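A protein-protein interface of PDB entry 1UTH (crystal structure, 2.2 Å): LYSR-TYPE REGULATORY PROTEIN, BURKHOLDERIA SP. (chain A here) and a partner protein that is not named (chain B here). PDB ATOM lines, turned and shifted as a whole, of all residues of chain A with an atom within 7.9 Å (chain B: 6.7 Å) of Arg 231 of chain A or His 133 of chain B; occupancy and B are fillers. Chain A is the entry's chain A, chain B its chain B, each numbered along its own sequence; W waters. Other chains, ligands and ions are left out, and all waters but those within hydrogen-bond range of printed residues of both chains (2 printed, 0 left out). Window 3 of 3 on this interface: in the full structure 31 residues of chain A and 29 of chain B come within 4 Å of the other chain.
The backbone carbonyl oxygen of His 133 of chain B lies within hydrogen-bond range of the guanidinium group of Arg 231 of chain A (3.3 Å). O of Arg 231 of chain A lies within hydrogen-bond range of N of Ile 136 of chain B (3.0 Å). The side-chain amide oxygen (OE1) of Gln 135 of chain B sits close to the backbone carbonyl oxygen (O) of Met 230 of chain A (2.9 Å). The guanidinium group (NE) of Arg 231 of chain A lies within hydrogen-bond range of the backbone carbonyl oxygen (O) of Pro 132 of chain B (3.5 Å). N of Val 233 of chain A lies within hydrogen-bond range of O of Ile 136 of chain B. The backbone carbonyl oxygen (O) of Ile 134 of chain B is in hydrogen-bond range of the guanidinium group (NH1) of Arg 231 of chain A (3.2 Å).
N of Gly 206 of chain A lies within hydrogen-bond range of O of Leu 232 of chain A, at 2.9 Å. The backbone NH of Gln 135 of chain B lies within hydrogen-bond range of the backbone carbonyl oxygen of Arg 105 of chain B (3.0 Å). The backbone carbonyl oxygen of His 204 of chain A sits at hydrogen-bond distance from the backbone NH of Arg 231 of chain A, at 3.1 Å. O of Phe 101 of chain B is in hydrogen-bond range of ND1 of His 133 of chain B, 3.3 Å away. SD of Met 230 of chain A sits close to NE of Arg 228 of chain A (3.7 Å). The backbone carbonyl oxygen (O) of His 204 of chain A is in hydrogen-bond range of the backbone NH (N) of Leu 232 of chain A, 3.4 Å away.
CA of Gln 135 of chain B touches O of Arg 231 of chain A, at 3.5 Å. CG of Leu 232 of chain A touches SD of Met 124 of chain B, at 3.9 Å. Leu 232 of chain A touches Ile 136 of chain B (CA to O, 3.2 Å). Val 233 of chain A touches Ser 137 of chain B.
Printed residues of chain B within 4 Å of Arg 231 of chain A: Pro 132 (3.5 Å), His 133 (3.3 Å), Ile 134 (3.2 Å), Gln 135 (3.5 Å) and Ile 136 (3.0 Å). Of chain A, only Arg 231 comes within 4 Å of His 133 of chain B. Printed residues of chain A within 4 Å of Ser 137 of chain B: Val 233. Printed residues of chain A within 4 Å of Gln 135 of chain B: Met 230 (2.9 Å) and Arg 231 (3.5 Å). The nearest residue of chain B that does not touch Arg 231 of chain A is Met 124 of chain B (4.03 Å). The nearest residue of chain A that does not touch His 133 of chain B is Arg 229 of chain A (5.3 Å).
Printed residues of chain A that touch a printed residue of chain B: Met 230, Arg 231, Leu 232 and Val 233. Hydrophobic or aromatic side chains of chain A that line the printed part of chain B: Leu 232 and Val 233. Along chain A the printed residues that touch a printed residue of chain B span positions 230 to 233. Of the 16 printed residues of chain B, 7 touch a printed residue of chain A. Hydrophobic or aromatic side chains of chain B that line the printed part of chain A: Met 124 and Ile 136.
Water W2 lies within hydrogen-bond range of the backbone carbonyl oxygen (O) of His 133 of chain B and the guanidinium group (NH1) of Arg 231 of chain A. Water W1 lies within hydrogen-bond range of the backbone carbonyl oxygen of Met 230 of chain A (2.9 Å) and the backbone carbonyl oxygen of Ile 136 of chain B (3.2 Å).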
ATOM      1  N   LEU A 202      25.307  17.809  31.809  1.00  0.00           N
ATOM      2  CA  LEU A 202      25.668  17.521  30.423  1.00  0.00           C
ATOM      3  C   LEU A 202      25.276  16.074  30.016  1.00  0.00           C
ATOM      4  O   LEU A 202      24.861  15.257  30.855  1.00  0.00           O
ATOM      5  CB  LEU A 202      27.163  17.778  30.252  1.00  0.00           C
ATOM      6  CG  LEU A 202      27.624  19.107  29.628  1.00  0.00           C
ATOM      7  CD1 LEU A 202      26.528  20.142  29.643  1.00  0.00           C
ATOM      8  CD2 LEU A 202      28.947  19.610  30.235  1.00  0.00           C
ATOM      9  N   GLU A 203      25.387  15.797  28.726  1.00  0.00           N
ATOM     10  CA  GLU A 203      25.130  14.468  28.169  1.00  0.00           C
ATOM     11  C   GLU A 203      26.408  13.639  27.868  1.00  0.00           C
ATOM     12  O   GLU A 203      27.389  14.159  27.373  1.00  0.00           O
ATOM     13  CB  GLU A 203      24.301  14.618  26.893  1.00  0.00           C
ATOM     14  CG  GLU A 203      22.885  15.041  27.197  1.00  0.00           C
ATOM     15  CD  GLU A 203      22.047  15.301  25.967  1.00  0.00           C
ATOM     16  OE1 GLU A 203      22.517  15.932  24.972  1.00  0.00           O
ATOM     17  OE2 GLU A 203      20.889  14.895  26.022  1.00  0.00           O
ATOM     18  N   HIS A 204      26.320  12.335  28.112  1.00  0.00           N
ATOM     19  CA  HIS A 204      27.470  11.438  28.131  1.00  0.00           C
ATOM     20  C   HIS A 204      27.453  10.349  27.060  1.00  0.00           C
ATOM     21  O   HIS A 204      26.393   9.835  26.698  1.00  0.00           O
ATOM     22  CB  HIS A 204      27.538  10.699  29.465  1.00  0.00           C
ATOM     23  CG  HIS A 204      27.624  11.597  30.653  1.00  0.00           C
ATOM     24  ND1 HIS A 204      28.628  11.486  31.588  1.00  0.00           N
ATOM     25  CD2 HIS A 204      26.828  12.612  31.067  1.00  0.00           C
ATOM     26  CE1 HIS A 204      28.442  12.393  32.534  1.00  0.00           C
ATOM     27  NE2 HIS A 204      27.358  13.085  32.241  1.00  0.00           N
ATOM     28  N   VAL A 205      28.653   9.993  26.613  1.00  0.00           N
ATOM     29  CA  VAL A 205      28.927   8.663  26.058  1.00  0.00           C
ATOM     30  C   VAL A 205      29.579   7.800  27.089  1.00  0.00           C
ATOM     31  O   VAL A 205      30.672   8.132  27.514  1.00  0.00           O
ATOM     32  CB  VAL A 205      30.028   8.595  24.966  1.00  0.00           C
ATOM     33  CG1 VAL A 205      29.649   7.566  23.919  1.00  0.00           C
ATOM     34  CG2 VAL A 205      30.469   9.899  24.433  1.00  0.00           C
ATOM     35  N   GLY A 206      28.965   6.659  27.395  1.00  0.00           N
ATOM     36  CA  GLY A 206      29.537   5.623  28.238  1.00  0.00           C
ATOM     37  C   GLY A 206      30.224   4.469  27.496  1.00  0.00           C
ATOM     38  O   GLY A 206      29.863   4.134  26.349  1.00  0.00           O
ATOM     39  N   ARG A 228      23.620  10.498  35.451  1.00  0.00           N
ATOM     40  CA  ARG A 228      24.088  10.823  34.112  1.00  0.00           C
ATOM     41  C   ARG A 228      23.028  10.485  33.096  1.00  0.00           C
ATOM     42  O   ARG A 228      22.482   9.385  33.111  1.00  0.00           O
ATOM     43  CB  ARG A 228      25.329  10.019  33.766  1.00  0.00           C
ATOM     44  CG  ARG A 228      26.577  10.363  34.542  1.00  0.00           C
ATOM     45  CD  ARG A 228      27.763   9.528  34.108  1.00  0.00           C
ATOM     46  NE  ARG A 228      27.524   8.111  34.390  1.00  0.00           N
ATOM     47  CZ  ARG A 228      28.164   7.113  33.801  1.00  0.00           C
ATOM     48  NH1 ARG A 228      29.112   7.347  32.916  1.00  0.00           N
ATOM     49  NH2 ARG A 228      27.877   5.877  34.138  1.00  0.00           N
ATOM     50  N   ARG A 229      22.762  11.429  32.202  1.00  0.00           N
ATOM     51  CA  ARG A 229      21.964  11.157  31.023  1.00  0.00           C
ATOM     52  C   ARG A 229      22.877  10.444  29.983  1.00  0.00           C
ATOM     53  O   ARG A 229      23.719  11.056  29.307  1.00  0.00           O
ATOM     54  CB  ARG A 229      21.326  12.442  30.444  1.00  0.00           C
ATOM     55  CG  ARG A 229      21.084  13.587  31.472  1.00  0.00           C
ATOM     56  CD  ARG A 229      19.930  14.545  31.153  1.00  0.00           C
ATOM     57  NE  ARG A 229      20.371  15.850  30.619  1.00  0.00           N
ATOM     58  CZ  ARG A 229      20.042  16.342  29.406  1.00  0.00           C
ATOM     59  NH1 ARG A 229      19.273  15.645  28.566  1.00  0.00           N
ATOM     60  NH2 ARG A 229      20.490  17.538  29.027  1.00  0.00           N
ATOM     61  N   MET A 230      22.713   9.135  29.908  1.00  0.00           N
ATOM     62  CA  MET A 230      23.489   8.282  29.015  1.00  0.00           C
ATOM     63  C   MET A 230      22.856   8.314  27.640  1.00  0.00           C
ATOM     64  O   MET A 230      21.964   7.554  27.335  1.00  0.00           O
ATOM     65  CB  MET A 230      23.519   6.853  29.572  1.00  0.00           C
ATOM     66  CG  MET A 230      24.090   6.710  31.007  1.00  0.00           C
ATOM     67  SD  MET A 230      25.749   7.446  31.228  1.00  0.00           S
ATOM     68  CE  MET A 230      26.621   6.836  29.817  1.00  0.00           C
ATOM     69  N   ARG A 231      23.319   9.213  26.812  1.00  0.00           N
ATOM     70  CA  ARG A 231      22.782   9.394  25.487  1.00  0.00           C
ATOM     71  C   ARG A 231      23.242   8.285  24.495  1.00  0.00           C
ATOM     72  O   ARG A 231      22.470   7.847  23.648  1.00  0.00           O
ATOM     73  CB  ARG A 231      23.248  10.760  25.017  1.00  0.00           C
ATOM     74  CG  ARG A 231      22.613  11.262  23.828  1.00  0.00           C
ATOM     75  CD  ARG A 231      21.072  11.239  23.927  1.00  0.00           C
ATOM     76  NE  ARG A 231      20.510  12.183  24.925  1.00  0.00           N
ATOM     77  CZ  ARG A 231      19.514  11.913  25.797  1.00  0.00           C
ATOM     78  NH1 ARG A 231      18.935  10.719  25.842  1.00  0.00           N
ATOM     79  NH2 ARG A 231      19.093  12.857  26.646  1.00  0.00           N
ATOM     80  N   LEU A 232      24.517   7.874  24.602  1.00  0.00           N
ATOM     81  CA  LEU A 232      25.123   6.801  23.806  1.00  0.00           C
ATOM     82  C   LEU A 232      25.907   5.869  24.748  1.00  0.00           C
ATOM     83  O   LEU A 232      26.616   6.342  25.675  1.00  0.00           O
ATOM     84  CB  LEU A 232      26.104   7.396  22.797  1.00  0.00           C
ATOM     85  CG  LEU A 232      26.513   6.670  21.506  1.00  0.00           C
ATOM     86  CD1 LEU A 232      27.950   6.871  21.179  1.00  0.00           C
ATOM     87  CD2 LEU A 232      26.093   5.192  21.361  1.00  0.00           C
ATOM     88  N   VAL A 233      25.781   4.570  24.531  1.00  0.00           N
ATOM     89  CA  VAL A 233      26.602   3.568  25.230  1.00  0.00           C
ATOM     90  C   VAL A 233      27.269   2.679  24.157  1.00  0.00           C
ATOM     91  O   VAL A 233      26.577   2.105  23.319  1.00  0.00           O
ATOM     92  CB  VAL A 233      25.753   2.737  26.231  1.00  0.00           C
ATOM     93  CG1 VAL A 233      26.492   1.473  26.712  1.00  0.00           C
ATOM     94  CG2 VAL A 233      25.345   3.595  27.458  1.00  0.00           C
ATOM     95  N   VAL A 234      28.597   2.587  24.197  1.00  0.00           N
ATOM     96  CA  VAL A 234      29.386   1.714  23.335  1.00  0.00           C
ATOM     97  C   VAL A 234      30.161   0.691  24.190  1.00  0.00           C
ATOM     98  O   VAL A 234      30.456   0.962  25.358  1.00  0.00           O
ATOM     99  CB  VAL A 234      30.357   2.527  22.460  1.00  0.00           C
ATOM    100  CG1 VAL A 234      29.588   3.383  21.454  1.00  0.00           C
ATOM    101  CG2 VAL A 234      31.323   3.448  23.323  1.00  0.00           C
ATOM    102  N   LEU A 249      28.759  15.822  23.568  1.00  0.00           N
ATOM    103  CA  LEU A 249      28.846  14.769  24.598  1.00  0.00           C
ATOM    104  C   LEU A 249      30.137  14.877  25.386  1.00  0.00           C
ATOM    105  O   LEU A 249      31.108  15.455  24.919  1.00  0.00           O
ATOM    106  CB  LEU A 249      28.791  13.381  23.938  1.00  0.00           C
ATOM    107  CG  LEU A 249      27.464  12.665  23.666  1.00  0.00           C
ATOM    108  CD1 LEU A 249      26.267  13.543  23.760  1.00  0.00           C
ATOM    109  CD2 LEU A 249      27.469  11.875  22.336  1.00  0.00           C
ATOM    110  N   ILE A 250      30.147  14.284  26.577  1.00  0.00           N
ATOM    111  CA  ILE A 250      31.352  14.154  27.368  1.00  0.00           C
ATOM    112  C   ILE A 250      31.539  12.701  27.782  1.00  0.00           C
ATOM    113  O   ILE A 250      30.619  11.914  27.724  1.00  0.00           O
ATOM    114  CB  ILE A 250      31.320  15.095  28.630  1.00  0.00           C
ATOM    115  CG1 ILE A 250      30.306  14.615  29.656  1.00  0.00           C
ATOM    116  CG2 ILE A 250      31.028  16.542  28.222  1.00  0.00           C
ATOM    117  CD1 ILE A 250      30.332  15.472  30.963  1.00  0.00           C
ATOM    118  N   PRO B 100       9.635  11.808  16.971  1.00  0.00           N
ATOM    119  CA  PRO B 100      11.071  11.979  17.197  1.00  0.00           C
ATOM    120  C   PRO B 100      11.435  13.091  18.170  1.00  0.00           C
ATOM    121  O   PRO B 100      12.480  13.003  18.788  1.00  0.00           O
ATOM    122  CB  PRO B 100      11.609  12.314  15.798  1.00  0.00           C
ATOM    123  CG  PRO B 100      10.418  12.868  15.051  1.00  0.00           C
ATOM    124  CD  PRO B 100       9.250  12.107  15.578  1.00  0.00           C
ATOM    125  N   PHE B 101      10.641  14.144  18.260  1.00  0.00           N
ATOM    126  CA  PHE B 101      10.920  15.205  19.228  1.00  0.00           C
ATOM    127  C   PHE B 101      10.686  14.756  20.701  1.00  0.00           C
ATOM    128  O   PHE B 101      11.328  15.267  21.606  1.00  0.00           O
ATOM    129  CB  PHE B 101      10.064  16.448  18.936  1.00  0.00           C
ATOM    130  CG  PHE B 101      10.386  17.150  17.642  1.00  0.00           C
ATOM    131  CD1 PHE B 101      11.414  16.735  16.805  1.00  0.00           C
ATOM    132  CD2 PHE B 101       9.640  18.250  17.271  1.00  0.00           C
ATOM    133  CE1 PHE B 101      11.683  17.429  15.643  1.00  0.00           C
ATOM    134  CE2 PHE B 101       9.921  18.953  16.116  1.00  0.00           C
ATOM    135  CZ  PHE B 101      10.934  18.534  15.293  1.00  0.00           C
ATOM    136  N   ALA B 102       9.802  13.792  20.921  1.00  0.00           N
ATOM    137  CA  ALA B 102       9.412  13.383  22.276  1.00  0.00           C
ATOM    138  C   ALA B 102       9.887  11.988  22.727  1.00  0.00           C
ATOM    139  O   ALA B 102       9.897  11.695  23.943  1.00  0.00           O
ATOM    140  CB  ALA B 102       7.895  13.429  22.394  1.00  0.00           C
ATOM    141  N   SER B 103      10.245  11.113  21.779  1.00  0.00           N
ATOM    142  CA  SER B 103      10.618   9.737  22.130  1.00  0.00           C
ATOM    143  C   SER B 103      11.803   9.694  23.096  1.00  0.00           C
ATOM    144  O   SER B 103      12.749  10.436  22.940  1.00  0.00           O
ATOM    145  CB  SER B 103      10.983   8.905  20.878  1.00  0.00           C
ATOM    146  OG  SER B 103      11.087   7.515  21.223  1.00  0.00           O
ATOM    147  N   THR B 104      11.711   8.804  24.076  1.00  0.00           N
ATOM    148  CA  THR B 104      12.798   8.460  24.989  1.00  0.00           C
ATOM    149  C   THR B 104      13.204   6.990  24.782  1.00  0.00           C
ATOM    150  O   THR B 104      13.856   6.418  25.620  1.00  0.00           O
ATOM    151  CB  THR B 104      12.330   8.619  26.472  1.00  0.00           C
ATOM    152  OG1 THR B 104      11.130   7.858  26.696  1.00  0.00           O
ATOM    153  CG2 THR B 104      11.928  10.091  26.813  1.00  0.00           C
ATOM    154  N   ARG B 105      12.794   6.386  23.672  1.00  0.00           N
ATOM    155  CA  ARG B 105      13.158   5.002  23.350  1.00  0.00           C
ATOM    156  C   ARG B 105      14.665   4.809  23.249  1.00  0.00           C
ATOM    157  O   ARG B 105      15.378   5.709  22.857  1.00  0.00           O
ATOM    158  CB  ARG B 105      12.516   4.596  22.044  1.00  0.00           C
ATOM    159  CG  ARG B 105      12.748   3.154  21.624  1.00  0.00           C
ATOM    160  CD  ARG B 105      11.698   2.670  20.653  1.00  0.00           C
ATOM    161  NE  ARG B 105      12.154   1.629  19.744  1.00  0.00           N
ATOM    162  CZ  ARG B 105      11.454   1.207  18.677  1.00  0.00           C
ATOM    163  NH1 ARG B 105      10.275   1.747  18.362  1.00  0.00           N
ATOM    164  NH2 ARG B 105      11.955   0.234  17.916  1.00  0.00           N
ATOM    165  N   MET B 124      25.291  10.679  15.727  1.00  0.00           N
ATOM    166  CA  MET B 124      24.956  11.313  17.002  1.00  0.00           C
ATOM    167  C   MET B 124      24.818  12.813  16.769  1.00  0.00           C
ATOM    168  O   MET B 124      23.932  13.409  17.268  1.00  0.00           O
ATOM    169  CB  MET B 124      25.982  11.014  18.091  1.00  0.00           C
ATOM    170  CG  MET B 124      26.031   9.576  18.570  1.00  0.00           C
ATOM    171  SD  MET B 124      24.500   8.804  18.990  1.00  0.00           S
ATOM    172  CE  MET B 124      23.888   9.854  20.272  1.00  0.00           C
ATOM    173  N   LEU B 127      21.293  13.128  15.392  1.00  0.00           N
ATOM    174  CA  LEU B 127      20.269  12.879  16.378  1.00  0.00           C
ATOM    175  C   LEU B 127      20.099  14.076  17.364  1.00  0.00           C
ATOM    176  O   LEU B 127      19.019  14.281  17.916  1.00  0.00           O
ATOM    177  CB  LEU B 127      20.574  11.593  17.139  1.00  0.00           C
ATOM    178  CG  LEU B 127      20.389  10.239  16.464  1.00  0.00           C
ATOM    179  CD1 LEU B 127      20.712   9.128  17.468  1.00  0.00           C
ATOM    180  CD2 LEU B 127      18.982  10.028  15.890  1.00  0.00           C
ATOM    181  N   ARG B 130      17.572  16.208  15.876  1.00  0.00           N
ATOM    182  CA  ARG B 130      16.365  15.570  15.399  1.00  0.00           C
ATOM    183  C   ARG B 130      15.566  14.730  16.390  1.00  0.00           C
ATOM    184  O   ARG B 130      14.337  14.571  16.251  1.00  0.00           O
ATOM    185  CB  ARG B 130      16.747  14.613  14.268  1.00  0.00           C
ATOM    186  CG  ARG B 130      17.228  15.259  13.008  1.00  0.00           C
ATOM    187  CD  ARG B 130      17.371  14.248  11.849  1.00  0.00           C
ATOM    188  NE  ARG B 130      18.360  14.698  10.867  1.00  0.00           N
ATOM    189  CZ  ARG B 130      18.241  14.530   9.560  1.00  0.00           C
ATOM    190  NH1 ARG B 130      17.184  13.912   9.042  1.00  0.00           N
ATOM    191  NH2 ARG B 130      19.203  14.984   8.775  1.00  0.00           N
ATOM    192  N   ALA B 131      16.242  14.136  17.348  1.00  0.00           N
ATOM    193  CA  ALA B 131      15.562  13.260  18.289  1.00  0.00           C
ATOM    194  C   ALA B 131      16.344  13.330  19.595  1.00  0.00           C
ATOM    195  O   ALA B 131      16.997  12.369  19.980  1.00  0.00           O
ATOM    196  CB  ALA B 131      15.485  11.854  17.752  1.00  0.00           C
ATOM    197  N   PRO B 132      16.253  14.485  20.268  1.00  0.00           N
ATOM    198  CA  PRO B 132      17.161  14.810  21.374  1.00  0.00           C
ATOM    199  C   PRO B 132      17.019  13.982  22.640  1.00  0.00           C
ATOM    200  O   PRO B 132      17.946  13.998  23.432  1.00  0.00           O
ATOM    201  CB  PRO B 132      16.926  16.309  21.648  1.00  0.00           C
ATOM    202  CG  PRO B 132      15.835  16.771  20.713  1.00  0.00           C
ATOM    203  CD  PRO B 132      15.284  15.560  19.994  1.00  0.00           C
ATOM    204  N   HIS B 133      15.966  13.203  22.774  1.00  0.00           N
ATOM    205  CA  HIS B 133      15.732  12.448  23.987  1.00  0.00           C
ATOM    206  C   HIS B 133      15.848  10.950  23.835  1.00  0.00           C
ATOM    207  O   HIS B 133      15.794  10.258  24.830  1.00  0.00           O
ATOM    208  CB  HIS B 133      14.372  12.845  24.563  1.00  0.00           C
ATOM    209  CG  HIS B 133      14.264  14.324  24.782  1.00  0.00           C
ATOM    210  ND1 HIS B 133      13.271  15.092  24.216  1.00  0.00           N
ATOM    211  CD2 HIS B 133      15.104  15.185  25.402  1.00  0.00           C
ATOM    212  CE1 HIS B 133      13.471  16.361  24.533  1.00  0.00           C
ATOM    213  NE2 HIS B 133      14.583  16.446  25.241  1.00  0.00           N
ATOM    214  N   ILE B 134      16.054  10.439  22.618  1.00  0.00           N
ATOM    215  CA  ILE B 134      16.286   8.988  22.484  1.00  0.00           C
ATOM    216  C   ILE B 134      17.697   8.610  22.950  1.00  0.00           C
ATOM    217  O   ILE B 134      18.604   9.425  22.982  1.00  0.00           O
ATOM    218  CB  ILE B 134      16.084   8.452  21.029  1.00  0.00           C
ATOM    219  CG1 ILE B 134      17.094   9.073  20.074  1.00  0.00           C
ATOM    220  CG2 ILE B 134      14.644   8.649  20.543  1.00  0.00           C
ATOM    221  CD1 ILE B 134      17.284   8.256  18.826  1.00  0.00           C
ATOM    222  N   GLN B 135      17.861   7.346  23.266  1.00  0.00           N
ATOM    223  CA  GLN B 135      19.152   6.813  23.653  1.00  0.00           C
ATOM    224  C   GLN B 135      19.552   5.745  22.632  1.00  0.00           C
ATOM    225  O   GLN B 135      18.696   5.063  22.076  1.00  0.00           O
ATOM    226  CB  GLN B 135      19.054   6.220  25.073  1.00  0.00           C
ATOM    227  CG  GLN B 135      18.499   7.192  26.235  1.00  0.00           C
ATOM    228  CD  GLN B 135      18.474   6.480  27.625  1.00  0.00           C
ATOM    229  OE1 GLN B 135      19.509   6.319  28.241  1.00  0.00           O
ATOM    230  NE2 GLN B 135      17.325   5.980  28.036  1.00  0.00           N
ATOM    231  N   ILE B 136      20.854   5.605  22.413  1.00  0.00           N
ATOM    232  CA  ILE B 136      21.420   4.590  21.542  1.00  0.00           C
ATOM    233  C   ILE B 136      22.427   3.738  22.338  1.00  0.00           C
ATOM    234  O   ILE B 136      23.196   4.297  23.138  1.00  0.00           O
ATOM    235  CB  ILE B 136      22.159   5.280  20.395  1.00  0.00           C
ATOM    236  CG1 ILE B 136      21.248   6.240  19.615  1.00  0.00           C
ATOM    237  CG2 ILE B 136      22.822   4.270  19.511  1.00  0.00           C
ATOM    238  CD1 ILE B 136      20.080   5.636  18.810  1.00  0.00           C
ATOM    239  N   SER B 137      22.417   2.416  22.148  1.00  0.00           N
ATOM    240  CA  SER B 137      23.535   1.560  22.550  1.00  0.00           C
ATOM    241  C   SER B 137      23.902   0.536  21.488  1.00  0.00           C
ATOM    242  O   SER B 137      23.045   0.051  20.761  1.00  0.00           O
ATOM    243  CB  SER B 137      23.286   0.848  23.879  1.00  0.00           C
ATOM    244  OG  SER B 137      22.061   0.170  23.833  1.00  0.00           O
HETATM  245  O   HOH W   1      22.049   4.898  26.070  1.00  0.00           O
HETATM  246  O   HOH W   2      16.043  10.488  27.529  1.00  0.00           O
